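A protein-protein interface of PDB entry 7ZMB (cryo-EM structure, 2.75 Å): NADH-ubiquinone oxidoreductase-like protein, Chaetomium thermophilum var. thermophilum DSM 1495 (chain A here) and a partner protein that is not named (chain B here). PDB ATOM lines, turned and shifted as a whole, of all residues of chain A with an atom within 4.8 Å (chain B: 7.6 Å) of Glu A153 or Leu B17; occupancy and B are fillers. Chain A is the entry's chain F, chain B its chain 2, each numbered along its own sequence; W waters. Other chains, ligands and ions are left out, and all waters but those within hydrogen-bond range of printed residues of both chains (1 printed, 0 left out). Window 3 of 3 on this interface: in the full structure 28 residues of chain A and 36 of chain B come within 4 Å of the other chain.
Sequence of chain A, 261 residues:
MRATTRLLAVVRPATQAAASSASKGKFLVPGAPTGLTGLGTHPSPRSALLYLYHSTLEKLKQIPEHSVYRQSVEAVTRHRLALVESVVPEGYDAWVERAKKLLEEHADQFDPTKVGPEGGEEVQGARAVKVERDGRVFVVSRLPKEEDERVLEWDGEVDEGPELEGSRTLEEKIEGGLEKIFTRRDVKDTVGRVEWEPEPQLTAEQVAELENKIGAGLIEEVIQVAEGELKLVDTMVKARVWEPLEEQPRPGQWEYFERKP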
ATOM      1  N   VAL A 151      11.336  -2.720 -19.934  1.00  0.00           N
ATOM      2  CA  VAL A 151      10.793  -3.659 -18.957  1.00  0.00           C
ATOM      3  C   VAL A 151       9.629  -3.031 -18.206  1.00  0.00           C
ATOM      4  O   VAL A 151       9.401  -3.341 -17.032  1.00  0.00           O
ATOM      5  CB  VAL A 151      11.871  -4.153 -17.969  1.00  0.00           C
ATOM      6  CG1 VAL A 151      12.893  -5.019 -18.690  1.00  0.00           C
ATOM      7  CG2 VAL A 151      12.543  -2.992 -17.267  1.00  0.00           C
ATOM      8  N   LEU A 152       8.879  -2.155 -18.866  1.00  0.00           N
ATOM      9  CA  LEU A 152       7.744  -1.481 -18.242  1.00  0.00           C
ATOM     10  C   LEU A 152       6.493  -1.756 -19.059  1.00  0.00           C
ATOM     11  O   LEU A 152       6.348  -1.240 -20.171  1.00  0.00           O
ATOM     12  CB  LEU A 152       7.993   0.019 -18.121  1.00  0.00           C
ATOM     13  CG  LEU A 152       7.014   0.764 -17.223  1.00  0.00           C
ATOM     14  CD1 LEU A 152       7.130   0.263 -15.810  1.00  0.00           C
ATOM     15  CD2 LEU A 152       7.272   2.246 -17.293  1.00  0.00           C
ATOM     16  N   GLU A 153       5.583  -2.542 -18.473  1.00  0.00           N
ATOM     17  CA  GLU A 153       4.365  -2.976 -19.206  1.00  0.00           C
ATOM     18  C   GLU A 153       3.197  -2.056 -18.868  1.00  0.00           C
ATOM     19  O   GLU A 153       3.005  -1.785 -17.672  1.00  0.00           O
ATOM     20  CB  GLU A 153       4.030  -4.431 -18.892  1.00  0.00           C
ATOM     21  CG  GLU A 153       5.109  -5.411 -19.289  1.00  0.00           C
ATOM     22  CD  GLU A 153       4.847  -6.788 -18.714  1.00  0.00           C
ATOM     23  OE1 GLU A 153       5.634  -7.712 -18.990  1.00  0.00           O
ATOM     24  OE2 GLU A 153       3.850  -6.925 -17.985  1.00  0.00           O
ATOM     25  N   TRP A 154       2.471  -1.585 -19.883  1.00  0.00           N
ATOM     26  CA  TRP A 154       1.279  -0.716 -19.693  1.00  0.00           C
ATOM     27  C   TRP A 154       1.613   0.548 -18.896  1.00  0.00           C
ATOM     28  O   TRP A 154       0.789   0.919 -18.055  1.00  0.00           O
ATOM     29  CB  TRP A 154       0.121  -1.504 -19.084  1.00  0.00           C
ATOM     30  CG  TRP A 154      -0.305  -2.668 -19.924  1.00  0.00           C
ATOM     31  CD1 TRP A 154      -0.934  -2.618 -21.133  1.00  0.00           C
ATOM     32  CD2 TRP A 154      -0.129  -4.064 -19.624  1.00  0.00           C
ATOM     33  NE1 TRP A 154      -1.174  -3.881 -21.599  1.00  0.00           N
ATOM     34  CE2 TRP A 154      -0.692  -4.789 -20.695  1.00  0.00           C
ATOM     35  CE3 TRP A 154       0.435  -4.769 -18.556  1.00  0.00           C
ATOM     36  CZ2 TRP A 154      -0.696  -6.182 -20.729  1.00  0.00           C
ATOM     37  CZ3 TRP A 154       0.430  -6.145 -18.591  1.00  0.00           C
ATOM     38  CH2 TRP A 154      -0.124  -6.838 -19.666  1.00  0.00           C
ATOM     39  N   ASP A 155       2.791   1.139 -19.118  1.00  0.00           N
ATOM     40  CA  ASP A 155       3.196   2.399 -18.443  1.00  0.00           C
ATOM     41  C   ASP A 155       3.453   2.149 -16.960  1.00  0.00           C
ATOM     42  O   ASP A 155       3.642   3.137 -16.233  1.00  0.00           O
ATOM     43  CB  ASP A 155       2.181   3.525 -18.654  1.00  0.00           C
ATOM     44  CG  ASP A 155       1.987   3.897 -20.113  1.00  0.00           C
ATOM     45  OD1 ASP A 155       2.980   3.855 -20.860  1.00  0.00           O
ATOM     46  OD2 ASP A 155       0.843   4.210 -20.489  1.00  0.00           O
ATOM     47  N   GLY A 156       3.494   0.888 -16.529  1.00  0.00           N
ATOM     48  CA  GLY A 156       3.596   0.642 -15.109  1.00  0.00           C
ATOM     49  C   GLY A 156       2.280   0.453 -14.404  1.00  0.00           C
ATOM     50  O   GLY A 156       2.240   0.511 -13.172  1.00  0.00           O
ATOM     51  N   GLU A 157       1.196   0.238 -15.149  1.00  0.00           N
ATOM     52  CA  GLU A 157      -0.136  -0.004 -14.535  1.00  0.00           C
ATOM     53  C   GLU A 157      -0.054  -1.164 -13.538  1.00  0.00           C
ATOM     54  O   GLU A 157       0.790  -2.040 -13.725  1.00  0.00           O
ATOM     55  CB  GLU A 157      -1.180  -0.185 -15.635  1.00  0.00           C
ATOM     56  CG  GLU A 157      -2.610  -0.241 -15.134  1.00  0.00           C
ATOM     57  CD  GLU A 157      -3.636   0.225 -16.149  1.00  0.00           C
ATOM     58  OE1 GLU A 157      -3.292   0.300 -17.345  1.00  0.00           O
ATOM     59  OE2 GLU A 157      -4.769   0.533 -15.735  1.00  0.00           O
ATOM     60  N   SER B  12      12.129 -10.011 -32.927  1.00  0.00           N
ATOM     61  CA  SER B  12      11.543  -8.895 -32.145  1.00  0.00           C
ATOM     62  C   SER B  12      11.035  -9.444 -30.820  1.00  0.00           C
ATOM     63  O   SER B  12      11.210  -8.767 -29.801  1.00  0.00           O
ATOM     64  CB  SER B  12      10.479  -8.199 -32.920  1.00  0.00           C
ATOM     65  OG  SER B  12      10.887  -8.029 -34.264  1.00  0.00           O
ATOM     66  N   THR B  13      10.433 -10.630 -30.846  1.00  0.00           N
ATOM     67  CA  THR B  13       9.902 -11.276 -29.619  1.00  0.00           C
ATOM     68  C   THR B  13      11.048 -11.607 -28.669  1.00  0.00           C
ATOM     69  O   THR B  13      10.833 -11.494 -27.458  1.00  0.00           O
ATOM     70  CB  THR B  13       9.101 -12.529 -29.989  1.00  0.00           C
ATOM     71  OG1 THR B  13       8.026 -12.103 -30.826  1.00  0.00           O
ATOM     72  CG2 THR B  13       8.550 -13.275 -28.794  1.00  0.00           C
ATOM     73  N   SER B  14      12.230 -11.940 -29.186  1.00  0.00           N
ATOM     74  CA  SER B  14      13.339 -12.434 -28.337  1.00  0.00           C
ATOM     75  C   SER B  14      14.087 -11.321 -27.587  1.00  0.00           C
ATOM     76  O   SER B  14      14.910 -11.659 -26.736  1.00  0.00           O
ATOM     77  CB  SER B  14      14.285 -13.211 -29.196  1.00  0.00           C
ATOM     78  OG  SER B  14      14.962 -12.359 -30.103  1.00  0.00           O
ATOM     79  N   VAL B  15      13.797 -10.055 -27.860  1.00  0.00           N
ATOM     80  CA  VAL B  15      14.444  -8.980 -27.122  1.00  0.00           C
ATOM     81  C   VAL B  15      13.447  -8.200 -26.266  1.00  0.00           C
ATOM     82  O   VAL B  15      13.724  -7.084 -25.860  1.00  0.00           O
ATOM     83  CB  VAL B  15      15.230  -8.049 -28.060  1.00  0.00           C
ATOM     84  CG1 VAL B  15      16.414  -8.785 -28.656  1.00  0.00           C
ATOM     85  CG2 VAL B  15      14.338  -7.521 -29.160  1.00  0.00           C
ATOM     86  N   THR B  16      12.291  -8.785 -25.975  1.00  0.00           N
ATOM     87  CA  THR B  16      11.290  -8.163 -25.125  1.00  0.00           C
ATOM     88  C   THR B  16      10.702  -9.205 -24.193  1.00  0.00           C
ATOM     89  O   THR B  16      10.507 -10.359 -24.582  1.00  0.00           O
ATOM     90  CB  THR B  16      10.166  -7.494 -25.955  1.00  0.00           C
ATOM     91  OG1 THR B  16       9.210  -6.872 -25.089  1.00  0.00           O
ATOM     92  CG2 THR B  16       9.455  -8.496 -26.845  1.00  0.00           C
ATOM     93  N   LEU B  17      10.451  -8.803 -22.952  1.00  0.00           N
ATOM     94  CA  LEU B  17       9.572  -9.549 -22.060  1.00  0.00           C
ATOM     95  C   LEU B  17       8.344  -8.732 -21.679  1.00  0.00           C
ATOM     96  O   LEU B  17       7.690  -9.030 -20.676  1.00  0.00           O
ATOM     97  CB  LEU B  17      10.315 -10.025 -20.810  1.00  0.00           C
ATOM     98  CG  LEU B  17      11.135 -11.319 -20.880  1.00  0.00           C
ATOM     99  CD1 LEU B  17      10.226 -12.517 -21.152  1.00  0.00           C
ATOM    100  CD2 LEU B  17      12.260 -11.263 -21.889  1.00  0.00           C
ATOM    101  N   ARG B  18       8.020  -7.708 -22.467  1.00  0.00           N
ATOM    102  CA  ARG B  18       6.864  -6.854 -22.218  1.00  0.00           C
ATOM    103  C   ARG B  18       5.611  -7.574 -22.683  1.00  0.00           C
ATOM    104  O   ARG B  18       5.431  -7.806 -23.880  1.00  0.00           O
ATOM    105  CB  ARG B  18       7.012  -5.523 -22.946  1.00  0.00           C
ATOM    106  CG  ARG B  18       7.908  -4.522 -22.267  1.00  0.00           C
ATOM    107  CD  ARG B  18       8.123  -3.328 -23.145  1.00  0.00           C
ATOM    108  NE  ARG B  18       6.856  -2.766 -23.597  1.00  0.00           N
ATOM    109  CZ  ARG B  18       6.688  -1.505 -23.978  1.00  0.00           C
ATOM    110  NH1 ARG B  18       7.705  -0.662 -23.968  1.00  0.00           N
ATOM    111  NH2 ARG B  18       5.502  -1.090 -24.374  1.00  0.00           N
ATOM    112  N   ARG B  19       4.711  -7.900 -21.753  1.00  0.00           N
ATOM    113  CA  ARG B  19       3.462  -8.636 -22.087  1.00  0.00           C
ATOM    114  C   ARG B  19       2.465  -7.731 -22.818  1.00  0.00           C
ATOM    115  O   ARG B  19       1.561  -8.280 -23.464  1.00  0.00           O
ATOM    116  CB  ARG B  19       2.852  -9.270 -20.837  1.00  0.00           C
ATOM    117  CG  ARG B  19       3.680 -10.408 -20.260  1.00  0.00           C
ATOM    118  CD  ARG B  19       3.105 -10.834 -18.928  1.00  0.00           C
ATOM    119  NE  ARG B  19       2.955  -9.684 -18.049  1.00  0.00           N
ATOM    120  CZ  ARG B  19       2.286  -9.698 -16.907  1.00  0.00           C
ATOM    121  NH1 ARG B  19       1.698 -10.808 -16.500  1.00  0.00           N
ATOM    122  NH2 ARG B  19       2.202  -8.599 -16.179  1.00  0.00           N
ATOM    123  N   ASP B  20       2.633  -6.413 -22.737  1.00  0.00           N
ATOM    124  CA  ASP B  20       1.753  -5.431 -23.420  1.00  0.00           C
ATOM    125  C   ASP B  20       1.948  -5.513 -24.940  1.00  0.00           C
ATOM    126  O   ASP B  20       1.109  -4.961 -25.666  1.00  0.00           O
ATOM    127  CB  ASP B  20       1.985  -4.025 -22.859  1.00  0.00           C
ATOM    128  CG  ASP B  20       3.400  -3.491 -22.953  1.00  0.00           C
ATOM    129  OD1 ASP B  20       4.282  -4.235 -23.396  1.00  0.00           O
ATOM    130  OD2 ASP B  20       3.599  -2.322 -22.583  1.00  0.00           O
ATOM    131  N   MET B  21       3.037  -6.134 -25.396  1.00  0.00           N
ATOM    132  CA  MET B  21       3.340  -6.270 -26.843  1.00  0.00           C
ATOM    133  C   MET B  21       2.517  -7.366 -27.521  1.00  0.00           C
ATOM    134  O   MET B  21       2.535  -7.387 -28.753  1.00  0.00           O
ATOM    135  CB  MET B  21       4.819  -6.609 -27.043  1.00  0.00           C
ATOM    136  CG  MET B  21       5.745  -5.424 -26.852  1.00  0.00           C
ATOM    137  SD  MET B  21       5.320  -4.026 -27.915  1.00  0.00           S
ATOM    138  CE  MET B  21       5.573  -4.733 -29.542  1.00  0.00           C
ATOM    139  N   MET B 116      -5.669  -6.695 -19.562  1.00  0.00           N
ATOM    140  CA  MET B 116      -4.675  -7.614 -18.954  1.00  0.00           C
ATOM    141  C   MET B 116      -5.206  -9.049 -18.927  1.00  0.00           C
ATOM    142  O   MET B 116      -4.728  -9.822 -18.093  1.00  0.00           O
ATOM    143  CB  MET B 116      -4.290  -7.128 -17.557  1.00  0.00           C
ATOM    144  CG  MET B 116      -4.132  -5.627 -17.508  1.00  0.00           C
ATOM    145  SD  MET B 116      -2.741  -5.060 -16.513  1.00  0.00           S
ATOM    146  CE  MET B 116      -2.705  -3.338 -16.998  1.00  0.00           C
ATOM    147  N   LYS B 121      -1.976 -11.542 -23.145  1.00  0.00           N
ATOM    148  CA  LYS B 121      -0.663 -11.430 -22.454  1.00  0.00           C
ATOM    149  C   LYS B 121       0.347 -12.506 -22.882  1.00  0.00           C
ATOM    150  O   LYS B 121       1.469 -12.467 -22.355  1.00  0.00           O
ATOM    151  CB  LYS B 121      -0.862 -11.444 -20.937  1.00  0.00           C
ATOM    152  CG  LYS B 121      -1.460 -10.182 -20.334  1.00  0.00           C
ATOM    153  CD  LYS B 121      -1.337 -10.147 -18.829  1.00  0.00           C
ATOM    154  CE  LYS B 121      -1.861 -11.400 -18.162  1.00  0.00           C
ATOM    155  NZ  LYS B 121      -1.876 -11.264 -16.688  1.00  0.00           N
ATOM    156  N   ILE B 123       3.062 -13.467 -25.229  1.00  0.00           N
ATOM    157  CA  ILE B 123       3.889 -12.815 -26.290  1.00  0.00           C
ATOM    158  C   ILE B 123       4.105 -13.749 -27.487  1.00  0.00           C
ATOM    159  O   ILE B 123       3.917 -13.278 -28.618  1.00  0.00           O
ATOM    160  CB  ILE B 123       5.214 -12.304 -25.687  1.00  0.00           C
ATOM    161  CG1 ILE B 123       5.012 -11.780 -24.263  1.00  0.00           C
ATOM    162  CG2 ILE B 123       5.858 -11.262 -26.586  1.00  0.00           C
ATOM    163  CD1 ILE B 123       6.274 -11.281 -23.605  1.00  0.00           C
ATOM    164  N   GLU B 124       4.318 -14.980 -27.332  1.00  0.00           N
ATOM    165  CA  GLU B 124       4.749 -15.963 -28.359  1.00  0.00           C
ATOM    166  C   GLU B 124       3.548 -16.615 -29.055  1.00  0.00           C
ATOM    167  O   GLU B 124       3.777 -17.387 -29.985  1.00  0.00           O
ATOM    168  CB  GLU B 124       5.676 -17.011 -27.732  1.00  0.00           C
ATOM    169  CG  GLU B 124       6.897 -16.436 -27.033  1.00  0.00           C
ATOM    170  CD  GLU B 124       6.721 -15.956 -25.598  1.00  0.00           C
ATOM    171  OE1 GLU B 124       7.740 -15.648 -24.960  1.00  0.00           O
ATOM    172  OE2 GLU B 124       5.572 -15.892 -25.120  1.00  0.00           O
HETATM  173  O   HOH W   1      -1.015  -2.958 -24.437  1.00  0.00           O
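The side-chain carboxylate of Glu A153 is in salt-bridge range of the guanidinium group of Arg B19 (2.9 Å).
The side-chain carboxylate (OD2) of Asp B20 is in hydrogen-bond range of the backbone NH (N) of Trp A154.
O of Leu B17 sits close to OE1 of Glu A153 (3.0 Å).
OG1 of Thr B16 lies within hydrogen-bond range of N of Arg B18 (3.0 Å).
The guanidinium group (NH2) of Arg B18 lies within salt-bridge range of the side-chain carboxylate (OD2) of Asp B20, at 2.9 Å.
The side-chain amino group (NZ) of Lys B121 lies close to the backbone carbonyl oxygen (O) of Met B116, 3.5 Å away.
Leu A152 touches Arg B18 (O to NE, 3.8 Å).
Leu A152 touches Asp B20.
Arg B18 touches Glu A153.
OD2 of Asp B20 touches CA of Glu A153, at 3.5 Å.
Arg B19 touches Trp A154.
Trp A154 touches Met B116 (CD2 to CE, 3.7 Å).
CH2 of Trp A154 touches CD of Lys B121 (3.6 Å).
Glu A157 touches Met B116 (CG to CE, 3.6 Å).
Glu A153 touches just these residues of chain B: Leu B17, Arg B18, Arg B19 and Asp B20.
Leu B17 touches one residue of chain A.
Printed residues of chain B within 4 Å of Glu A157: Met B116.
Of the printed residues of chain A, Met B116 touches Trp A154 and Glu A157.
Printed residues of chain A within 4 Å of Asp B20: Leu A152, Glu A153 and Trp A154.
Printed residues of chain A within 4 Å of Arg B18: Leu A152 (3.8 Å) and Glu A153 (3.6 Å).
Of the printed residues of chain A, Lys B121 touches Trp A154.
Val A151 touches none of the printed residues of chain B.
Asp A155 touches none of the printed residues of chain B.
The nearest printed residue of chain A that does not touch Lys B121 is Glu A153 (6.2 Å).
Along chain B the printed residues that touch a printed residue of chain A span positions 17 to 121.
Hydrophobic or aromatic side chains of chain A within 4 Å of the printed part of chain B: Trp A154.
Among the printed residues, 11 pairs touch across the chains.
Water W1 bridges NE1 of Trp A154 and O of Asp B20.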
